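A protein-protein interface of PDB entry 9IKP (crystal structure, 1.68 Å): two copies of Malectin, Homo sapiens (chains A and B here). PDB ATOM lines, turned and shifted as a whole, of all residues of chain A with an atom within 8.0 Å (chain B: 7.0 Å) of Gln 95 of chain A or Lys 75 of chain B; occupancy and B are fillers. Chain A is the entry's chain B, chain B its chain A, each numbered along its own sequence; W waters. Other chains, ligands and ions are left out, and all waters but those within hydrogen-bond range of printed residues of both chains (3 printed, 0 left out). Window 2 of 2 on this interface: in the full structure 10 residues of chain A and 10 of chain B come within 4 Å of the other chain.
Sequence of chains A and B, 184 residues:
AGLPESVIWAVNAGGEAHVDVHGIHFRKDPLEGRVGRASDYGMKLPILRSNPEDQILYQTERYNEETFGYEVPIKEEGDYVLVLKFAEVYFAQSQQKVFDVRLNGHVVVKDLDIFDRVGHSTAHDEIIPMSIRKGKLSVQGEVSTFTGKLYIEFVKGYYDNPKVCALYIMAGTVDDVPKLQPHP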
ATOM      1  N   PHE A  91       4.578 -22.236  -4.580  1.00  0.00           N
ATOM      2  CA  PHE A  91       6.044 -22.311  -4.567  1.00  0.00           C
ATOM      3  C   PHE A  91       6.710 -20.944  -4.326  1.00  0.00           C
ATOM      4  O   PHE A  91       6.114 -19.881  -4.542  1.00  0.00           O
ATOM      5  CB  PHE A  91       6.554 -22.912  -5.890  1.00  0.00           C
ATOM      6  CG  PHE A  91       6.154 -24.357  -6.099  1.00  0.00           C
ATOM      7  CD1 PHE A  91       6.724 -25.361  -5.324  1.00  0.00           C
ATOM      8  CD2 PHE A  91       5.201 -24.704  -7.049  1.00  0.00           C
ATOM      9  CE1 PHE A  91       6.382 -26.698  -5.520  1.00  0.00           C
ATOM     10  CE2 PHE A  91       4.830 -26.038  -7.240  1.00  0.00           C
ATOM     11  CZ  PHE A  91       5.416 -27.037  -6.470  1.00  0.00           C
ATOM     12  N   ALA A  92       7.978 -20.992  -3.867  1.00  0.00           N
ATOM     13  CA  ALA A  92       8.808 -19.809  -3.575  1.00  0.00           C
ATOM     14  C   ALA A  92      10.292 -20.056  -3.918  1.00  0.00           C
ATOM     15  O   ALA A  92      11.202 -19.538  -3.248  1.00  0.00           O
ATOM     16  CB  ALA A  92       8.657 -19.375  -2.111  1.00  0.00           C
ATOM     17  N   GLN A  93      10.548 -20.815  -4.992  1.00  0.00           N
ATOM     18  CA  GLN A  93      11.869 -21.007  -5.603  1.00  0.00           C
ATOM     19  C   GLN A  93      11.694 -21.124  -7.121  1.00  0.00           C
ATOM     20  O   GLN A  93      10.598 -21.423  -7.606  1.00  0.00           O
ATOM     21  CB  GLN A  93      12.601 -22.263  -5.076  1.00  0.00           C
ATOM     22  CG  GLN A  93      12.828 -22.302  -3.539  1.00  0.00           C
ATOM     23  CD  GLN A  93      13.560 -23.567  -3.068  1.00  0.00           C
ATOM     24  OE1 GLN A  93      14.797 -23.592  -2.983  1.00  0.00           O
ATOM     25  NE2 GLN A  93      12.799 -24.605  -2.715  1.00  0.00           N
ATOM     26  N   SER A  94      12.777 -20.881  -7.877  1.00  0.00           N
ATOM     27  CA  SER A  94      12.705 -21.027  -9.335  1.00  0.00           C
ATOM     28  C   SER A  94      12.805 -22.503  -9.754  1.00  0.00           C
ATOM     29  O   SER A  94      13.219 -23.377  -8.980  1.00  0.00           O
ATOM     30  CB  SER A  94      13.789 -20.187 -10.031  1.00  0.00           C
ATOM     31  OG  SER A  94      15.053 -20.843 -10.030  1.00  0.00           O
ATOM     32  N   GLN A  95      12.359 -22.774 -10.994  1.00  0.00           N
ATOM     33  CA  GLN A  95      12.331 -24.119 -11.596  1.00  0.00           C
ATOM     34  C   GLN A  95      11.596 -25.147 -10.724  1.00  0.00           C
ATOM     35  O   GLN A  95      12.019 -26.306 -10.593  1.00  0.00           O
ATOM     36  CB  GLN A  95      13.749 -24.596 -11.939  1.00  0.00           C
ATOM     37  CG  GLN A  95      13.785 -25.685 -12.994  1.00  0.00           C
ATOM     38  CD  GLN A  95      15.075 -25.689 -13.776  1.00  0.00           C
ATOM     39  OE1 GLN A  95      16.160 -25.802 -13.202  1.00  0.00           O
ATOM     40  NE2 GLN A  95      14.969 -25.552 -15.097  1.00  0.00           N
ATOM     41  N   GLN A  96      10.466 -24.731 -10.137  1.00  0.00           N
ATOM     42  CA  GLN A  96       9.542 -25.631  -9.444  1.00  0.00           C
ATOM     43  C   GLN A  96       8.286 -25.901 -10.269  1.00  0.00           C
ATOM     44  O   GLN A  96       7.883 -27.070 -10.396  1.00  0.00           O
ATOM     45  CB  GLN A  96       9.150 -25.078  -8.057  1.00  0.00           C
ATOM     46  CG  GLN A  96      10.340 -24.686  -7.157  1.00  0.00           C
ATOM     47  CD  GLN A  96      11.233 -25.858  -6.715  1.00  0.00           C
ATOM     48  OE1 GLN A  96      10.798 -26.788  -6.011  1.00  0.00           O
ATOM     49  NE2 GLN A  96      12.514 -25.797  -7.113  1.00  0.00           N
ATOM     50  N   LYS A  97       7.645 -24.851 -10.815  1.00  0.00           N
ATOM     51  CA  LYS A  97       6.528 -24.945 -11.772  1.00  0.00           C
ATOM     52  C   LYS A  97       6.906 -24.171 -13.038  1.00  0.00           C
ATOM     53  O   LYS A  97       7.158 -22.961 -12.964  1.00  0.00           O
ATOM     54  CB  LYS A  97       5.228 -24.372 -11.172  1.00  0.00           C
ATOM     55  CG  LYS A  97       3.998 -24.395 -12.122  1.00  0.00           C
ATOM     56  CD  LYS A  97       2.811 -23.473 -11.666  1.00  0.00           C
ATOM     57  CE  LYS A  97       2.085 -23.896 -10.373  1.00  0.00           C
ATOM     58  NZ  LYS A  97       1.316 -25.192 -10.552  1.00  0.00           N
ATOM     59  N   VAL A  98       6.948 -24.866 -14.194  1.00  0.00           N
ATOM     60  CA  VAL A  98       7.321 -24.295 -15.503  1.00  0.00           C
ATOM     61  C   VAL A  98       6.450 -24.923 -16.603  1.00  0.00           C
ATOM     62  O   VAL A  98       6.297 -26.150 -16.636  1.00  0.00           O
ATOM     63  CB  VAL A  98       8.819 -24.540 -15.822  1.00  0.00           C
ATOM     64  CG1 VAL A  98       9.244 -23.806 -17.106  1.00  0.00           C
ATOM     65  CG2 VAL A  98       9.737 -24.150 -14.645  1.00  0.00           C
ATOM     66  N   ASP A 111       8.556 -21.682 -21.670  1.00  0.00           N
ATOM     67  CA  ASP A 111       9.107 -21.903 -20.319  1.00  0.00           C
ATOM     68  C   ASP A 111       8.700 -20.795 -19.335  1.00  0.00           C
ATOM     69  O   ASP A 111       9.552 -20.166 -18.685  1.00  0.00           O
ATOM     70  CB  ASP A 111      10.642 -22.049 -20.350  1.00  0.00           C
ATOM     71  CG  ASP A 111      11.128 -23.267 -21.155  1.00  0.00           C
ATOM     72  OD1 ASP A 111      10.446 -24.313 -21.173  1.00  0.00           O
ATOM     73  OD2 ASP A 111      12.231 -23.184 -21.749  1.00  0.00           O
ATOM     74  N   ASP A 113       7.819 -19.320 -15.995  1.00  0.00           N
ATOM     75  CA  ASP A 113       8.138 -19.598 -14.585  1.00  0.00           C
ATOM     76  C   ASP A 113       7.658 -18.382 -13.786  1.00  0.00           C
ATOM     77  O   ASP A 113       8.380 -17.381 -13.666  1.00  0.00           O
ATOM     78  CB  ASP A 113       9.697 -19.878 -14.434  1.00  0.00           C
ATOM     79  CG  ASP A 113      10.131 -20.272 -13.022  1.00  0.00           C
ATOM     80  OD1 ASP A 113       9.398 -20.010 -12.020  1.00  0.00           O
ATOM     81  OD2 ASP A 113      11.264 -20.843 -12.932  1.00  0.00           O
ATOM     82  N   ILE A 114       6.419 -18.463 -13.268  1.00  0.00           N
ATOM     83  CA  ILE A 114       5.781 -17.301 -12.639  1.00  0.00           C
ATOM     84  C   ILE A 114       6.616 -16.789 -11.458  1.00  0.00           C
ATOM     85  O   ILE A 114       6.868 -15.581 -11.342  1.00  0.00           O
ATOM     86  CB  ILE A 114       4.326 -17.624 -12.225  1.00  0.00           C
ATOM     87  CG1 ILE A 114       3.471 -18.071 -13.425  1.00  0.00           C
ATOM     88  CG2 ILE A 114       3.671 -16.405 -11.523  1.00  0.00           C
ATOM     89  CD1 ILE A 114       2.343 -19.057 -13.051  1.00  0.00           C
ATOM     90  N   PHE A 115       7.070 -17.683 -10.562  1.00  0.00           N
ATOM     91  CA  PHE A 115       7.869 -17.207  -9.429  1.00  0.00           C
ATOM     92  C   PHE A 115       9.129 -16.475  -9.892  1.00  0.00           C
ATOM     93  O   PHE A 115       9.482 -15.424  -9.341  1.00  0.00           O
ATOM     94  CB  PHE A 115       8.269 -18.343  -8.476  1.00  0.00           C
ATOM     95  CG  PHE A 115       9.202 -17.875  -7.379  1.00  0.00           C
ATOM     96  CD1 PHE A 115       8.699 -17.301  -6.217  1.00  0.00           C
ATOM     97  CD2 PHE A 115      10.580 -17.946  -7.544  1.00  0.00           C
ATOM     98  CE1 PHE A 115       9.559 -16.825  -5.225  1.00  0.00           C
ATOM     99  CE2 PHE A 115      11.460 -17.459  -6.550  1.00  0.00           C
ATOM    100  CZ  PHE A 115      10.944 -16.906  -5.402  1.00  0.00           C
ATOM    101  N   ASP A 116       9.843 -17.019 -10.891  1.00  0.00           N
ATOM    102  CA  ASP A 116      11.090 -16.376 -11.325  1.00  0.00           C
ATOM    103  C   ASP A 116      10.849 -14.930 -11.766  1.00  0.00           C
ATOM    104  O   ASP A 116      11.691 -14.058 -11.514  1.00  0.00           O
ATOM    105  CB  ASP A 116      11.749 -17.195 -12.454  1.00  0.00           C
ATOM    106  CG  ASP A 116      13.221 -16.810 -12.729  1.00  0.00           C
ATOM    107  OD1 ASP A 116      14.043 -16.736 -11.778  1.00  0.00           O
ATOM    108  OD2 ASP A 116      13.585 -16.657 -13.925  1.00  0.00           O
ATOM    109  N   TYR A 158       7.778 -31.402 -17.316  1.00  0.00           N
ATOM    110  CA  TYR A 158       8.270 -32.126 -16.143  1.00  0.00           C
ATOM    111  C   TYR A 158       8.107 -31.387 -14.809  1.00  0.00           C
ATOM    112  O   TYR A 158       8.052 -32.055 -13.764  1.00  0.00           O
ATOM    113  CB  TYR A 158       9.758 -32.486 -16.304  1.00  0.00           C
ATOM    114  CG  TYR A 158      10.063 -33.673 -17.202  1.00  0.00           C
ATOM    115  CD1 TYR A 158      10.121 -34.965 -16.679  1.00  0.00           C
ATOM    116  CD2 TYR A 158      10.344 -33.505 -18.552  1.00  0.00           C
ATOM    117  CE1 TYR A 158      10.410 -36.060 -17.494  1.00  0.00           C
ATOM    118  CE2 TYR A 158      10.640 -34.594 -19.369  1.00  0.00           C
ATOM    119  CZ  TYR A 158      10.670 -35.865 -18.832  1.00  0.00           C
ATOM    120  OH  TYR A 158      10.964 -36.953 -19.635  1.00  0.00           O
ATOM    121  N   TYR A 159       8.042 -30.045 -14.796  1.00  0.00           N
ATOM    122  CA  TYR A 159       8.070 -29.257 -13.550  1.00  0.00           C
ATOM    123  C   TYR A 159       6.653 -28.824 -13.142  1.00  0.00           C
ATOM    124  O   TYR A 159       6.146 -27.795 -13.590  1.00  0.00           O
ATOM    125  CB  TYR A 159       8.988 -28.038 -13.721  1.00  0.00           C
ATOM    126  CG  TYR A 159      10.467 -28.356 -13.978  1.00  0.00           C
ATOM    127  CD1 TYR A 159      11.279 -28.835 -12.962  1.00  0.00           C
ATOM    128  CD2 TYR A 159      11.030 -28.188 -15.242  1.00  0.00           C
ATOM    129  CE1 TYR A 159      12.628 -29.129 -13.188  1.00  0.00           C
ATOM    130  CE2 TYR A 159      12.379 -28.490 -15.479  1.00  0.00           C
ATOM    131  CZ  TYR A 159      13.168 -28.954 -14.440  1.00  0.00           C
ATOM    132  OH  TYR A 159      14.506 -29.257 -14.664  1.00  0.00           O
ATOM    133  N   ASP A 160       6.019 -29.622 -12.284  1.00  0.00           N
ATOM    134  CA  ASP A 160       4.673 -29.428 -11.702  1.00  0.00           C
ATOM    135  C   ASP A 160       3.635 -29.209 -12.818  1.00  0.00           C
ATOM    136  O   ASP A 160       3.797 -29.722 -13.928  1.00  0.00           O
ATOM    137  CB  ASP A 160       4.714 -28.344 -10.631  1.00  0.00           C
ATOM    138  CG  ASP A 160       3.537 -28.440  -9.640  1.00  0.00           C
ATOM    139  OD1 ASP A 160       3.574 -29.313  -8.720  1.00  0.00           O
ATOM    140  OD2 ASP A 160       2.584 -27.616  -9.732  1.00  0.00           O
ATOM    141  N   ILE B   8      11.662 -19.665   1.747  1.00  0.00           N
ATOM    142  CA  ILE B   8      11.633 -20.535   0.565  1.00  0.00           C
ATOM    143  C   ILE B   8      10.652 -21.713   0.675  1.00  0.00           C
ATOM    144  O   ILE B   8      10.301 -22.297  -0.362  1.00  0.00           O
ATOM    145  CB  ILE B   8      13.047 -21.075   0.193  1.00  0.00           C
ATOM    146  CG1 ILE B   8      13.691 -21.906   1.318  1.00  0.00           C
ATOM    147  CG2 ILE B   8      14.004 -19.941  -0.170  1.00  0.00           C
ATOM    148  CD1 ILE B   8      14.734 -22.925   0.846  1.00  0.00           C
ATOM    149  N   PRO B  73      13.189 -29.735  -1.107  1.00  0.00           N
ATOM    150  CA  PRO B  73      14.123 -29.356  -2.189  1.00  0.00           C
ATOM    151  C   PRO B  73      14.739 -27.982  -1.927  1.00  0.00           C
ATOM    152  O   PRO B  73      14.022 -27.040  -1.577  1.00  0.00           O
ATOM    153  CB  PRO B  73      13.237 -29.321  -3.443  1.00  0.00           C
ATOM    154  CG  PRO B  73      11.820 -29.148  -2.940  1.00  0.00           C
ATOM    155  CD  PRO B  73      11.766 -29.568  -1.482  1.00  0.00           C
ATOM    156  N   ILE B  74      16.064 -27.859  -2.107  1.00  0.00           N
ATOM    157  CA  ILE B  74      16.763 -26.568  -2.004  1.00  0.00           C
ATOM    158  C   ILE B  74      17.489 -26.277  -3.323  1.00  0.00           C
ATOM    159  O   ILE B  74      18.431 -26.989  -3.698  1.00  0.00           O
ATOM    160  CB  ILE B  74      17.737 -26.520  -0.810  1.00  0.00           C
ATOM    161  CG1 ILE B  74      17.025 -26.981   0.466  1.00  0.00           C
ATOM    162  CG2 ILE B  74      18.345 -25.094  -0.643  1.00  0.00           C
ATOM    163  CD1 ILE B  74      17.759 -26.685   1.772  1.00  0.00           C
ATOM    164  N   LYS B  75      17.072 -25.196  -4.000  1.00  0.00           N
ATOM    165  CA  LYS B  75      17.478 -24.912  -5.377  1.00  0.00           C
ATOM    166  C   LYS B  75      18.856 -24.242  -5.488  1.00  0.00           C
ATOM    167  O   LYS B  75      19.591 -24.520  -6.446  1.00  0.00           O
ATOM    168  CB  LYS B  75      16.403 -24.034  -6.040  1.00  0.00           C
ATOM    169  CG  LYS B  75      16.681 -23.530  -7.458  1.00  0.00           C
ATOM    170  CD  LYS B  75      16.710 -24.666  -8.480  1.00  0.00           C
ATOM    171  CE  LYS B  75      16.875 -24.108  -9.892  1.00  0.00           C
ATOM    172  NZ  LYS B  75      18.245 -23.569 -10.115  1.00  0.00           N
ATOM    173  N   GLU B  76      19.227 -23.364  -4.552  1.00  0.00           N
ATOM    174  CA  GLU B  76      20.422 -22.534  -4.690  1.00  0.00           C
ATOM    175  C   GLU B  76      21.319 -22.644  -3.454  1.00  0.00           C
ATOM    176  O   GLU B  76      20.844 -22.887  -2.335  1.00  0.00           O
ATOM    177  CB  GLU B  76      20.026 -21.045  -4.920  1.00  0.00           C
ATOM    178  CG  GLU B  76      19.230 -20.746  -6.232  1.00  0.00           C
ATOM    179  CD  GLU B  76      19.995 -20.999  -7.530  1.00  0.00           C
ATOM    180  OE1 GLU B  76      21.245 -21.073  -7.519  1.00  0.00           O
ATOM    181  OE2 GLU B  76      19.332 -21.097  -8.590  1.00  0.00           O
ATOM    182  N   GLU B  77      22.632 -22.473  -3.666  1.00  0.00           N
ATOM    183  CA  GLU B  77      23.589 -22.382  -2.555  1.00  0.00           C
ATOM    184  C   GLU B  77      23.386 -21.096  -1.737  1.00  0.00           C
ATOM    185  O   GLU B  77      22.917 -20.073  -2.250  1.00  0.00           O
ATOM    186  CB  GLU B  77      25.033 -22.447  -3.086  1.00  0.00           C
ATOM    187  CG  GLU B  77      25.335 -23.734  -3.869  1.00  0.00           C
ATOM    188  CD  GLU B  77      26.789 -24.185  -3.820  1.00  0.00           C
ATOM    189  OE1 GLU B  77      27.703 -23.333  -3.727  1.00  0.00           O
ATOM    190  OE2 GLU B  77      27.011 -25.418  -3.883  1.00  0.00           O
ATOM    191  N   TYR B  80      21.228 -20.384   5.348  1.00  0.00           N
ATOM    192  CA  TYR B  80      19.803 -20.572   5.664  1.00  0.00           C
ATOM    193  C   TYR B  80      19.611 -20.801   7.168  1.00  0.00           C
ATOM    194  O   TYR B  80      20.555 -21.153   7.879  1.00  0.00           O
ATOM    195  CB  TYR B  80      19.208 -21.776   4.898  1.00  0.00           C
ATOM    196  CG  TYR B  80      19.207 -21.676   3.372  1.00  0.00           C
ATOM    197  CD1 TYR B  80      18.150 -21.065   2.701  1.00  0.00           C
ATOM    198  CD2 TYR B  80      20.252 -22.205   2.601  1.00  0.00           C
ATOM    199  CE1 TYR B  80      18.127 -20.969   1.323  1.00  0.00           C
ATOM    200  CE2 TYR B  80      20.235 -22.113   1.196  1.00  0.00           C
ATOM    201  CZ  TYR B  80      19.168 -21.487   0.569  1.00  0.00           C
ATOM    202  OH  TYR B  80      19.102 -21.380  -0.813  1.00  0.00           O
ATOM    203  N   PHE B 146      25.763 -32.948  -0.110  1.00  0.00           N
ATOM    204  CA  PHE B 146      24.383 -32.519  -0.373  1.00  0.00           C
ATOM    205  C   PHE B 146      23.995 -32.835  -1.813  1.00  0.00           C
ATOM    206  O   PHE B 146      24.689 -32.421  -2.750  1.00  0.00           O
ATOM    207  CB  PHE B 146      24.203 -31.015  -0.102  1.00  0.00           C
ATOM    208  CG  PHE B 146      22.749 -30.557  -0.089  1.00  0.00           C
ATOM    209  CD1 PHE B 146      21.876 -30.973   0.913  1.00  0.00           C
ATOM    210  CD2 PHE B 146      22.269 -29.715  -1.086  1.00  0.00           C
ATOM    211  CE1 PHE B 146      20.540 -30.550   0.911  1.00  0.00           C
ATOM    212  CE2 PHE B 146      20.941 -29.294  -1.103  1.00  0.00           C
ATOM    213  CZ  PHE B 146      20.077 -29.707  -0.111  1.00  0.00           C
ATOM    214  N   GLY B 148      20.746 -32.183  -3.164  1.00  0.00           N
ATOM    215  CA  GLY B 148      19.636 -31.375  -3.631  1.00  0.00           C
ATOM    216  C   GLY B 148      18.425 -31.396  -2.723  1.00  0.00           C
ATOM    217  O   GLY B 148      17.539 -30.537  -2.876  1.00  0.00           O
HETATM  218  O   HOH W   1      17.166 -19.357  -8.846  1.00  0.00           O
HETATM  219  O   HOH W   2      16.963 -21.853  -2.840  1.00  0.00           O
HETATM  220  O   HOH W   3       9.037 -23.446  -2.661  1.00  0.00           O
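N of Lys 75 of chain B is in hydrogen-bond range of OE1 of Gln 93 of chain A, at 3.0 Å. O of Pro 73 of chain B sits at hydrogen-bond distance from NE2 of Gln 93 of chain A (3.0 Å).
Among the printed residues, pairs that only touch across the chains: Gln 93 of chain A with Ile 74 of chain B (3.7 Å), Ser 94 of chain A with Lys 75 of chain B (3.7 Å), Gln 95 of chain A with Lys 75 of chain B (3.8 Å), Ala 92 of chain A with Ile 8 of chain B (3.8 Å) and Gln 93 of chain A with Ile 8 of chain B (3.9 Å).
No position is printed for both chains. Of the 7 pairs that touch across the chains among the printed residues, none has its exchanged pair printed and touching as well.
The backbone NH of Gln 95 of chain A lies within hydrogen-bond range of the side-chain carboxylate of Asp 113 of chain A (2.9 Å). O of Ser 94 of chain A sits at hydrogen-bond distance from NE2 of Gln 96 of chain A, 3.1 Å away. NZ of Lys 75 of chain B lies within salt-bridge range of OE2 of Glu 76 of chain B (3.1 Å). N of Ile 74 of chain B is in hydrogen-bond range of O of Gly 148 of chain B (3.2 Å).
Hydrophobic or aromatic side chains of chain A within 4 Å of the printed part of chain B: Ala 92. Of the 9 printed residues of chain B, 4 touch a printed residue of chain A. Hydrophobic or aromatic side chains of chain B within 4 Å of the printed part of chain A: Ile 8. Along chain B the printed residues that touch a printed residue of chain A span positions 8 to 75. Among the printed residues, 7 pairs touch across the chains. Among the printed residues, no Asp or Glu carboxylate lies within 4 Å of a Lys or Arg side-chain nitrogen of the other chain.
Printed residues of chain B within 4 Å of Ser 94 of chain A: Lys 75. Gln 95 of chain A touches one residue of chain B. Of the printed residues of chain A, Pro 73 of chain B touches Gln 93. Of chain A, only Gln 93 (3.0 Å), Ser 94 (3.7 Å) and Gln 95 (3.8 Å) come within 4 Å of Lys 75 of chain B. The nearest residue of chain A that does not touch Lys 75 of chain B is Gln 96 of chain A (4.4 Å).
Water W2 lies within hydrogen-bond range of the side-chain amide oxygen of Gln 93 of chain A (2.8 Å), the side-chain hydroxyl of Tyr 80 of chain B (3.0 Å) and the backbone NH of Glu 76 of chain B (3.2 Å). Water W1 lies within hydrogen-bond range of the side-chain carboxylate of Glu 76 of chain B (2.8 Å) and the side-chain hydroxyl of Ser 94 of chain A (2.8 Å). Water W3 bridges the backbone carbonyl oxygen (O) of Ile 8 of chain B (2.9 Å) and the backbone NH (N) of Ala 92 of chain A (2.9 Å).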
